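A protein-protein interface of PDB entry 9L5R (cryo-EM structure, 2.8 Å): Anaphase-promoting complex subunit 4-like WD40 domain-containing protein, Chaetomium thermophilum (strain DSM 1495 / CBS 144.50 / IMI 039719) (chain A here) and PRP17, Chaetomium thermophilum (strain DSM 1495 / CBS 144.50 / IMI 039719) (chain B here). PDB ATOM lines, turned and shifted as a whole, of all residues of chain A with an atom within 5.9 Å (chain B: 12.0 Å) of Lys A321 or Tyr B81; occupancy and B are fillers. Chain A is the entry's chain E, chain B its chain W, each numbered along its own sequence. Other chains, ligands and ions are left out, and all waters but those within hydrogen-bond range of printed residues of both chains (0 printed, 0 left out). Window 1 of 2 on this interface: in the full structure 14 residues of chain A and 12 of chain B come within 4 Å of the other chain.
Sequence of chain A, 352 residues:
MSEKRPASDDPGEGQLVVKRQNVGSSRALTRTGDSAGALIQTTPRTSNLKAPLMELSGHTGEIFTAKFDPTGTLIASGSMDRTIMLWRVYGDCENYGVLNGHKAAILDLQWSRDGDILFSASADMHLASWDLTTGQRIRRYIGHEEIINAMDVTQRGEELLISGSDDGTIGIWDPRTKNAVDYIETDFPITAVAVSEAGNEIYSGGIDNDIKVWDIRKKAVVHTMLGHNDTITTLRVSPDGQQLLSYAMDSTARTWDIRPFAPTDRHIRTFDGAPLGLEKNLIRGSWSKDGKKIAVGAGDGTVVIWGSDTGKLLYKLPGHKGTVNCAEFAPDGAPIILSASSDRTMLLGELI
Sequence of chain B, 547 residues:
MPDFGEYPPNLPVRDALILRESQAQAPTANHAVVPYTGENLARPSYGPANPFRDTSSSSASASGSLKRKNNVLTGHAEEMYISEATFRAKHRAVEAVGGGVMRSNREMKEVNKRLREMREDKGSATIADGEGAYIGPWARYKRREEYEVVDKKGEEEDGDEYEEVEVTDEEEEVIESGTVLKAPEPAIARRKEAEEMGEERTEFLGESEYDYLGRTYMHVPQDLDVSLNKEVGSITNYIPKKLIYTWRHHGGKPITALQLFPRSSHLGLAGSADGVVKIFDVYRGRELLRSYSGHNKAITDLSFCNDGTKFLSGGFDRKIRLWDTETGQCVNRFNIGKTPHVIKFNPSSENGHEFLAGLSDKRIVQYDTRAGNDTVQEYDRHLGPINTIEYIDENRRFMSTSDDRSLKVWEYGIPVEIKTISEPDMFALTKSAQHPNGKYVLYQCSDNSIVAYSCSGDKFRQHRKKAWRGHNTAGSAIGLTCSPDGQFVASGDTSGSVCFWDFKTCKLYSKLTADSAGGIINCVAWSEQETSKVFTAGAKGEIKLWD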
ATOM      1  N   GLU A  62      19.627 -24.296  -2.929  1.00  0.00           N
ATOM      2  CA  GLU A  62      20.222 -23.618  -4.075  1.00  0.00           C
ATOM      3  C   GLU A  62      21.321 -22.665  -3.630  1.00  0.00           C
ATOM      4  O   GLU A  62      21.133 -21.886  -2.696  1.00  0.00           O
ATOM      5  CB  GLU A  62      19.149 -22.845  -4.833  1.00  0.00           C
ATOM      6  CG  GLU A  62      17.931 -23.657  -5.257  1.00  0.00           C
ATOM      7  CD  GLU A  62      16.812 -23.677  -4.234  1.00  0.00           C
ATOM      8  OE1 GLU A  62      17.096 -23.665  -3.021  1.00  0.00           O
ATOM      9  OE2 GLU A  62      15.639 -23.682  -4.644  1.00  0.00           O
ATOM     10  N   GLU A 279      13.873 -20.112 -14.505  1.00  0.00           N
ATOM     11  CA  GLU A 279      13.965 -19.478 -13.200  1.00  0.00           C
ATOM     12  C   GLU A 279      14.413 -18.037 -13.382  1.00  0.00           C
ATOM     13  O   GLU A 279      15.362 -17.768 -14.123  1.00  0.00           O
ATOM     14  CB  GLU A 279      14.955 -20.220 -12.305  1.00  0.00           C
ATOM     15  CG  GLU A 279      14.623 -21.672 -12.061  1.00  0.00           C
ATOM     16  CD  GLU A 279      15.443 -22.263 -10.943  1.00  0.00           C
ATOM     17  OE1 GLU A 279      15.235 -21.872  -9.779  1.00  0.00           O
ATOM     18  OE2 GLU A 279      16.307 -23.115 -11.224  1.00  0.00           O
ATOM     19  N   GLY A 299      21.139 -20.755 -17.530  1.00  0.00           N
ATOM     20  CA  GLY A 299      20.115 -21.605 -16.954  1.00  0.00           C
ATOM     21  C   GLY A 299      20.089 -23.023 -17.472  1.00  0.00           C
ATOM     22  O   GLY A 299      19.456 -23.876 -16.840  1.00  0.00           O
ATOM     23  N   GLY A 301      22.499 -24.878 -17.172  1.00  0.00           N
ATOM     24  CA  GLY A 301      23.575 -25.482 -16.426  1.00  0.00           C
ATOM     25  C   GLY A 301      24.951 -25.155 -16.935  1.00  0.00           C
ATOM     26  O   GLY A 301      25.910 -25.837 -16.564  1.00  0.00           O
ATOM     27  N   GLY A 319      28.076 -28.634 -16.718  1.00  0.00           N
ATOM     28  CA  GLY A 319      28.386 -29.262 -15.451  1.00  0.00           C
ATOM     29  C   GLY A 319      27.331 -29.169 -14.377  1.00  0.00           C
ATOM     30  O   GLY A 319      27.464 -29.789 -13.321  1.00  0.00           O
ATOM     31  N   HIS A 320      26.279 -28.408 -14.626  1.00  0.00           N
ATOM     32  CA  HIS A 320      25.289 -28.137 -13.603  1.00  0.00           C
ATOM     33  C   HIS A 320      23.916 -28.552 -14.095  1.00  0.00           C
ATOM     34  O   HIS A 320      23.638 -28.545 -15.296  1.00  0.00           O
ATOM     35  CB  HIS A 320      25.301 -26.665 -13.207  1.00  0.00           C
ATOM     36  CG  HIS A 320      26.510 -26.272 -12.420  1.00  0.00           C
ATOM     37  ND1 HIS A 320      26.770 -26.767 -11.163  1.00  0.00           N
ATOM     38  CD2 HIS A 320      27.536 -25.442 -12.715  1.00  0.00           C
ATOM     39  CE1 HIS A 320      27.901 -26.257 -10.714  1.00  0.00           C
ATOM     40  NE2 HIS A 320      28.388 -25.452 -11.639  1.00  0.00           N
ATOM     41  N   LYS A 321      23.067 -28.940 -13.152  1.00  0.00           N
ATOM     42  CA  LYS A 321      21.737 -29.423 -13.464  1.00  0.00           C
ATOM     43  C   LYS A 321      20.648 -28.415 -13.145  1.00  0.00           C
ATOM     44  O   LYS A 321      19.501 -28.617 -13.551  1.00  0.00           O
ATOM     45  CB  LYS A 321      21.481 -30.737 -12.719  1.00  0.00           C
ATOM     46  CG  LYS A 321      22.497 -31.797 -13.087  1.00  0.00           C
ATOM     47  CD  LYS A 321      22.601 -32.880 -12.042  1.00  0.00           C
ATOM     48  CE  LYS A 321      23.536 -33.979 -12.502  1.00  0.00           C
ATOM     49  NZ  LYS A 321      24.879 -33.453 -12.859  1.00  0.00           N
ATOM     50  N   GLY A 322      20.976 -27.340 -12.442  1.00  0.00           N
ATOM     51  CA  GLY A 322      20.067 -26.227 -12.290  1.00  0.00           C
ATOM     52  C   GLY A 322      20.628 -25.012 -12.989  1.00  0.00           C
ATOM     53  O   GLY A 322      21.628 -25.127 -13.700  1.00  0.00           O
ATOM     54  N   THR A 323      19.999 -23.854 -12.817  1.00  0.00           N
ATOM     55  CA  THR A 323      20.552 -22.627 -13.364  1.00  0.00           C
ATOM     56  C   THR A 323      21.844 -22.300 -12.637  1.00  0.00           C
ATOM     57  O   THR A 323      21.960 -22.522 -11.433  1.00  0.00           O
ATOM     58  CB  THR A 323      19.573 -21.471 -13.213  1.00  0.00           C
ATOM     59  OG1 THR A 323      19.329 -21.246 -11.828  1.00  0.00           O
ATOM     60  CG2 THR A 323      18.253 -21.818 -13.856  1.00  0.00           C
ATOM     61  N   SER A 341      25.647 -23.157  -8.755  1.00  0.00           N
ATOM     62  CA  SER A 341      24.351 -23.352  -9.378  1.00  0.00           C
ATOM     63  C   SER A 341      23.288 -23.628  -8.331  1.00  0.00           C
ATOM     64  O   SER A 341      23.569 -23.788  -7.144  1.00  0.00           O
ATOM     65  CB  SER A 341      24.390 -24.508 -10.372  1.00  0.00           C
ATOM     66  OG  SER A 341      23.108 -24.740 -10.914  1.00  0.00           O
ATOM     67  N   SER A 342      22.051 -23.743  -8.804  1.00  0.00           N
ATOM     68  CA  SER A 342      20.975 -24.204  -7.948  1.00  0.00           C
ATOM     69  C   SER A 342      20.935 -25.725  -7.972  1.00  0.00           C
ATOM     70  O   SER A 342      19.874 -26.329  -8.109  1.00  0.00           O
ATOM     71  CB  SER A 342      19.649 -23.619  -8.412  1.00  0.00           C
ATOM     72  OG  SER A 342      19.201 -24.271  -9.578  1.00  0.00           O
ATOM     73  N   ASP A 343      22.101 -26.337  -7.793  1.00  0.00           N
ATOM     74  CA  ASP A 343      22.301 -27.768  -7.737  1.00  0.00           C
ATOM     75  C   ASP A 343      22.689 -28.224  -6.356  1.00  0.00           C
ATOM     76  O   ASP A 343      23.003 -29.407  -6.181  1.00  0.00           O
ATOM     77  CB  ASP A 343      23.418 -28.199  -8.686  1.00  0.00           C
ATOM     78  CG  ASP A 343      22.910 -28.688  -9.979  1.00  0.00           C
ATOM     79  OD1 ASP A 343      21.691 -28.878 -10.087  1.00  0.00           O
ATOM     80  OD2 ASP A 343      23.735 -28.935 -10.873  1.00  0.00           O
ATOM     81  N   ARG A 344      22.723 -27.304  -5.390  1.00  0.00           N
ATOM     82  CA  ARG A 344      23.315 -27.509  -4.071  1.00  0.00           C
ATOM     83  C   ARG A 344      24.789 -27.901  -4.164  1.00  0.00           C
ATOM     84  O   ARG A 344      25.324 -28.549  -3.263  1.00  0.00           O
ATOM     85  CB  ARG A 344      22.522 -28.532  -3.247  1.00  0.00           C
ATOM     86  CG  ARG A 344      21.020 -28.405  -3.392  1.00  0.00           C
ATOM     87  CD  ARG A 344      20.287 -29.408  -2.549  1.00  0.00           C
ATOM     88  NE  ARG A 344      18.883 -29.047  -2.418  1.00  0.00           N
ATOM     89  CZ  ARG A 344      17.884 -29.707  -2.981  1.00  0.00           C
ATOM     90  NH1 ARG A 344      18.094 -30.797  -3.697  1.00  0.00           N
ATOM     91  NH2 ARG A 344      16.643 -29.259  -2.823  1.00  0.00           N
ATOM     92  N   TYR B  36      35.268 -28.312 -24.643  1.00  0.00           N
ATOM     93  CA  TYR B  36      34.234 -27.301 -24.511  1.00  0.00           C
ATOM     94  C   TYR B  36      34.694 -25.943 -25.007  1.00  0.00           C
ATOM     95  O   TYR B  36      34.011 -24.944 -24.769  1.00  0.00           O
ATOM     96  CB  TYR B  36      33.791 -27.205 -23.057  1.00  0.00           C
ATOM     97  CG  TYR B  36      33.735 -28.536 -22.352  1.00  0.00           C
ATOM     98  CD1 TYR B  36      32.749 -29.460 -22.646  1.00  0.00           C
ATOM     99  CD2 TYR B  36      34.683 -28.872 -21.401  1.00  0.00           C
ATOM    100  CE1 TYR B  36      32.701 -30.674 -22.005  1.00  0.00           C
ATOM    101  CE2 TYR B  36      34.645 -30.080 -20.759  1.00  0.00           C
ATOM    102  CZ  TYR B  36      33.653 -30.977 -21.064  1.00  0.00           C
ATOM    103  OH  TYR B  36      33.612 -32.186 -20.420  1.00  0.00           O
ATOM    104  N   ASN B  71      16.556 -42.068 -23.366  1.00  0.00           N
ATOM    105  CA  ASN B  71      16.728 -43.061 -22.319  1.00  0.00           C
ATOM    106  C   ASN B  71      15.406 -43.577 -21.763  1.00  0.00           C
ATOM    107  O   ASN B  71      15.372 -44.669 -21.183  1.00  0.00           O
ATOM    108  CB  ASN B  71      17.618 -42.490 -21.207  1.00  0.00           C
ATOM    109  CG  ASN B  71      17.053 -41.224 -20.570  1.00  0.00           C
ATOM    110  OD1 ASN B  71      15.945 -40.786 -20.866  1.00  0.00           O
ATOM    111  ND2 ASN B  71      17.831 -40.635 -19.677  1.00  0.00           N
ATOM    112  N   HIS B  76      12.942 -38.183 -23.550  1.00  0.00           N
ATOM    113  CA  HIS B  76      14.179 -38.002 -22.807  1.00  0.00           C
ATOM    114  C   HIS B  76      13.861 -37.361 -21.466  1.00  0.00           C
ATOM    115  O   HIS B  76      13.232 -36.303 -21.418  1.00  0.00           O
ATOM    116  CB  HIS B  76      15.170 -37.139 -23.588  1.00  0.00           C
ATOM    117  CG  HIS B  76      16.526 -37.076 -22.967  1.00  0.00           C
ATOM    118  ND1 HIS B  76      17.319 -38.189 -22.800  1.00  0.00           N
ATOM    119  CD2 HIS B  76      17.231 -36.035 -22.468  1.00  0.00           C
ATOM    120  CE1 HIS B  76      18.452 -37.838 -22.224  1.00  0.00           C
ATOM    121  NE2 HIS B  76      18.424 -36.537 -22.010  1.00  0.00           N
ATOM    122  N   ALA B  77      14.292 -38.007 -20.386  1.00  0.00           N
ATOM    123  CA  ALA B  77      14.099 -37.504 -19.034  1.00  0.00           C
ATOM    124  C   ALA B  77      15.451 -37.215 -18.405  1.00  0.00           C
ATOM    125  O   ALA B  77      16.355 -38.052 -18.455  1.00  0.00           O
ATOM    126  CB  ALA B  77      13.331 -38.502 -18.177  1.00  0.00           C
ATOM    127  N   GLU B  78      15.583 -36.037 -17.808  1.00  0.00           N
ATOM    128  CA  GLU B  78      16.832 -35.616 -17.197  1.00  0.00           C
ATOM    129  C   GLU B  78      16.541 -35.088 -15.800  1.00  0.00           C
ATOM    130  O   GLU B  78      15.548 -34.389 -15.592  1.00  0.00           O
ATOM    131  CB  GLU B  78      17.508 -34.546 -18.061  1.00  0.00           C
ATOM    132  CG  GLU B  78      18.857 -34.079 -17.588  1.00  0.00           C
ATOM    133  CD  GLU B  78      19.465 -33.065 -18.534  1.00  0.00           C
ATOM    134  OE1 GLU B  78      18.805 -32.725 -19.537  1.00  0.00           O
ATOM    135  OE2 GLU B  78      20.604 -32.619 -18.286  1.00  0.00           O
ATOM    136  N   GLU B  79      17.393 -35.445 -14.844  1.00  0.00           N
ATOM    137  CA  GLU B  79      17.234 -34.947 -13.485  1.00  0.00           C
ATOM    138  C   GLU B  79      17.539 -33.457 -13.439  1.00  0.00           C
ATOM    139  O   GLU B  79      18.526 -32.995 -14.015  1.00  0.00           O
ATOM    140  CB  GLU B  79      18.140 -35.702 -12.520  1.00  0.00           C
ATOM    141  CG  GLU B  79      17.789 -35.445 -11.071  1.00  0.00           C
ATOM    142  CD  GLU B  79      18.927 -35.732 -10.124  1.00  0.00           C
ATOM    143  OE1 GLU B  79      20.094 -35.673 -10.558  1.00  0.00           O
ATOM    144  OE2 GLU B  79      18.655 -36.007  -8.939  1.00  0.00           O
ATOM    145  N   MET B  80      16.691 -32.704 -12.751  1.00  0.00           N
ATOM    146  CA  MET B  80      16.709 -31.256 -12.819  1.00  0.00           C
ATOM    147  C   MET B  80      16.569 -30.701 -11.408  1.00  0.00           C
ATOM    148  O   MET B  80      16.130 -31.391 -10.487  1.00  0.00           O
ATOM    149  CB  MET B  80      15.589 -30.762 -13.736  1.00  0.00           C
ATOM    150  CG  MET B  80      15.617 -29.310 -14.102  1.00  0.00           C
ATOM    151  SD  MET B  80      14.192 -29.016 -15.105  1.00  0.00           S
ATOM    152  CE  MET B  80      13.032 -29.321 -13.810  1.00  0.00           C
ATOM    153  N   TYR B  81      16.967 -29.449 -11.228  1.00  0.00           N
ATOM    154  CA  TYR B  81      17.070 -28.855  -9.908  1.00  0.00           C
ATOM    155  C   TYR B  81      16.475 -27.456  -9.886  1.00  0.00           C
ATOM    156  O   TYR B  81      17.107 -26.498  -9.443  1.00  0.00           O
ATOM    157  CB  TYR B  81      18.521 -28.834  -9.467  1.00  0.00           C
ATOM    158  CG  TYR B  81      18.982 -30.085  -8.777  1.00  0.00           C
ATOM    159  CD1 TYR B  81      18.844 -30.231  -7.410  1.00  0.00           C
ATOM    160  CD2 TYR B  81      19.561 -31.119  -9.493  1.00  0.00           C
ATOM    161  CE1 TYR B  81      19.274 -31.363  -6.776  1.00  0.00           C
ATOM    162  CE2 TYR B  81      19.994 -32.254  -8.868  1.00  0.00           C
ATOM    163  CZ  TYR B  81      19.847 -32.373  -7.508  1.00  0.00           C
ATOM    164  OH  TYR B  81      20.274 -33.509  -6.872  1.00  0.00           O
ATOM    165  N   ILE B  82      15.254 -27.304 -10.389  1.00  0.00           N
ATOM    166  CA  ILE B  82      14.571 -26.022 -10.270  1.00  0.00           C
ATOM    167  C   ILE B  82      14.081 -25.832  -8.846  1.00  0.00           C
ATOM    168  O   ILE B  82      14.132 -26.751  -8.023  1.00  0.00           O
ATOM    169  CB  ILE B  82      13.397 -25.880 -11.249  1.00  0.00           C
ATOM    170  CG1 ILE B  82      12.323 -26.922 -10.955  1.00  0.00           C
ATOM    171  CG2 ILE B  82      13.894 -25.948 -12.680  1.00  0.00           C
ATOM    172  CD1 ILE B  82      10.948 -26.447 -11.312  1.00  0.00           C
ATOM    173  N   SER B  83      13.616 -24.629  -8.551  1.00  0.00           N
ATOM    174  CA  SER B  83      13.145 -24.258  -7.231  1.00  0.00           C
ATOM    175  C   SER B  83      11.677 -24.618  -7.044  1.00  0.00           C
ATOM    176  O   SER B  83      10.886 -24.653  -7.996  1.00  0.00           O
ATOM    177  CB  SER B  83      13.349 -22.764  -7.005  1.00  0.00           C
ATOM    178  OG  SER B  83      12.789 -22.352  -5.780  1.00  0.00           O
ATOM    179  N   GLU B  84      11.326 -24.887  -5.786  1.00  0.00           N
ATOM    180  CA  GLU B  84       9.964 -25.275  -5.449  1.00  0.00           C
ATOM    181  C   GLU B  84       8.985 -24.148  -5.730  1.00  0.00           C
ATOM    182  O   GLU B  84       7.872 -24.387  -6.205  1.00  0.00           O
ATOM    183  CB  GLU B  84       9.904 -25.702  -3.985  1.00  0.00           C
ATOM    184  CG  GLU B  84       8.577 -26.289  -3.571  1.00  0.00           C
ATOM    185  CD  GLU B  84       8.357 -27.678  -4.121  1.00  0.00           C
ATOM    186  OE1 GLU B  84       9.299 -28.494  -4.066  1.00  0.00           O
ATOM    187  OE2 GLU B  84       7.245 -27.951  -4.612  1.00  0.00           O
ATOM    188  N   ALA B  85       9.393 -22.910  -5.450  1.00  0.00           N
ATOM    189  CA  ALA B  85       8.558 -21.755  -5.749  1.00  0.00           C
ATOM    190  C   ALA B  85       8.350 -21.597  -7.246  1.00  0.00           C
ATOM    191  O   ALA B  85       7.256 -21.232  -7.688  1.00  0.00           O
ATOM    192  CB  ALA B  85       9.187 -20.496  -5.164  1.00  0.00           C
ATOM    193  N   THR B  86       9.395 -21.860  -8.035  1.00  0.00           N
ATOM    194  CA  THR B  86       9.282 -21.822  -9.490  1.00  0.00           C
ATOM    195  C   THR B  86       8.245 -22.815  -9.984  1.00  0.00           C
ATOM    196  O   THR B  86       7.354 -22.460 -10.770  1.00  0.00           O
ATOM    197  CB  THR B  86      10.635 -22.125 -10.133  1.00  0.00           C
ATOM    198  OG1 THR B  86      11.603 -21.159  -9.718  1.00  0.00           O
ATOM    199  CG2 THR B  86      10.524 -22.099 -11.636  1.00  0.00           C
ATOM    200  N   PHE B  87       8.338 -24.064  -9.510  1.00  0.00           N
ATOM    201  CA  PHE B  87       7.372 -25.075  -9.927  1.00  0.00           C
ATOM    202  C   PHE B  87       5.961 -24.707  -9.501  1.00  0.00           C
ATOM    203  O   PHE B  87       5.018 -24.856 -10.283  1.00  0.00           O
ATOM    204  CB  PHE B  87       7.735 -26.453  -9.375  1.00  0.00           C
ATOM    205  CG  PHE B  87       6.817 -27.546  -9.855  1.00  0.00           C
ATOM    206  CD1 PHE B  87       7.084 -28.212 -11.033  1.00  0.00           C
ATOM    207  CD2 PHE B  87       5.679 -27.893  -9.142  1.00  0.00           C
ATOM    208  CE1 PHE B  87       6.241 -29.189 -11.483  1.00  0.00           C
ATOM    209  CE2 PHE B  87       4.834 -28.859  -9.603  1.00  0.00           C
ATOM    210  CZ  PHE B  87       5.116 -29.512 -10.765  1.00  0.00           C
ATOM    211  N   ARG B  88       5.796 -24.244  -8.261  1.00  0.00           N
ATOM    212  CA  ARG B  88       4.461 -23.945  -7.762  1.00  0.00           C
ATOM    213  C   ARG B  88       3.841 -22.776  -8.509  1.00  0.00           C
ATOM    214  O   ARG B  88       2.648 -22.799  -8.822  1.00  0.00           O
ATOM    215  CB  ARG B  88       4.517 -23.665  -6.267  1.00  0.00           C
ATOM    216  CG  ARG B  88       4.449 -24.905  -5.408  1.00  0.00           C
ATOM    217  CD  ARG B  88       4.880 -24.593  -4.000  1.00  0.00           C
ATOM    218  NE  ARG B  88       5.019 -25.785  -3.178  1.00  0.00           N
ATOM    219  CZ  ARG B  88       4.088 -26.231  -2.349  1.00  0.00           C
ATOM    220  NH1 ARG B  88       2.926 -25.615  -2.221  1.00  0.00           N
ATOM    221  NH2 ARG B  88       4.329 -27.325  -1.634  1.00  0.00           N
ATOM    222  N   LYS B  90       4.576 -21.726 -11.692  1.00  0.00           N
ATOM    223  CA  LYS B  90       4.230 -22.103 -13.060  1.00  0.00           C
ATOM    224  C   LYS B  90       3.021 -23.030 -13.092  1.00  0.00           C
ATOM    225  O   LYS B  90       2.135 -22.889 -13.952  1.00  0.00           O
ATOM    226  CB  LYS B  90       5.434 -22.747 -13.733  1.00  0.00           C
ATOM    227  CG  LYS B  90       6.534 -21.757 -13.994  1.00  0.00           C
ATOM    228  CD  LYS B  90       7.696 -22.372 -14.723  1.00  0.00           C
ATOM    229  CE  LYS B  90       8.783 -21.344 -14.950  1.00  0.00           C
ATOM    230  NZ  LYS B  90       8.287 -20.153 -15.680  1.00  0.00           N
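OE2 of Glu A62 sits at hydrogen-bond distance from OG of Ser B83, at 3.3 Å. OG of Ser A342 sits at hydrogen-bond distance from O of Tyr B81. The backbone NH (N) of Ser B83 is in hydrogen-bond range of the side-chain carboxylate (OE1) of Glu A279.
OD1 of Asp A343 sits at hydrogen-bond distance from N of Gly A322 (2.9 Å). The backbone NH (N) of Lys A321 lies close to the side-chain carboxylate (OD1) of Asp A343. The side-chain hydroxyl (OG) of Ser B83 sits close to the backbone NH (N) of Ala B85 (3.5 Å). The backbone carbonyl oxygen of Thr A323 is in hydrogen-bond range of the backbone NH of Ser A342 (2.9 Å).
Among the printed residues, merely in contact across the chains: Asp A343 with Tyr B81 (3.1 Å), Arg A344 with Tyr B81 (3.3 Å), Glu A279 with Ile B82 (3.5 Å), Lys A321 with Tyr B81 (3.5 Å), Glu A279 with Thr B86 (3.7 Å), Glu A279 with Tyr B81 (3.9 Å), Lys A321 with Met B80 (3.9 Å) and Lys A321 with Glu B79 (3.9 Å).
No residue of chain B comes within 4 Å of Gly A319. No residue of chain B comes within 4 Å of His A320. Of chain B, only Glu B79 (3.9 Å), Met B80 (3.9 Å) and Tyr B81 (3.5 Å) come within 4 Å of Lys A321. No residue of chain B comes within 4 Å of Gly A322. No residue of chain B comes within 4 Å of Thr A323. No residue of chain B comes within 4 Å of Ser A341. Of chain B, only Tyr B81 (3.1 Å) comes within 4 Å of Ser A342. Asp A343 touches one residue of chain B. Of the printed residues of chain A, Glu B79 touches Lys A321. Of chain A, only Glu A279, Lys A321, Ser A342, Asp A343 and Arg A344 come within 4 Å of Tyr B81. Of the printed residues of chain A, Ile B82 touches Glu A279 (3.5 Å). Of the printed residues of chain A, Thr B86 touches Glu A279. Arg B88 touches none of the printed residues of chain A. The nearest residue of chain A that does not touch Tyr B81 is Gly A322 (4.1 Å). The nearest printed residue of chain A that does not touch Ser B83 is Ser A342 (5.7 Å).
Printed residues of chain B that touch a printed residue of chain A: Glu B79, Met B80, Tyr B81, Ile B82, Ser B83 and Thr B86. Hydrophobic or aromatic side chains of chain B within 4 Å of the printed part of chain A: Met B80, Tyr B81 and Ile B82. Of the 13 printed residues of chain A, 6 touch a printed residue of chain B.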
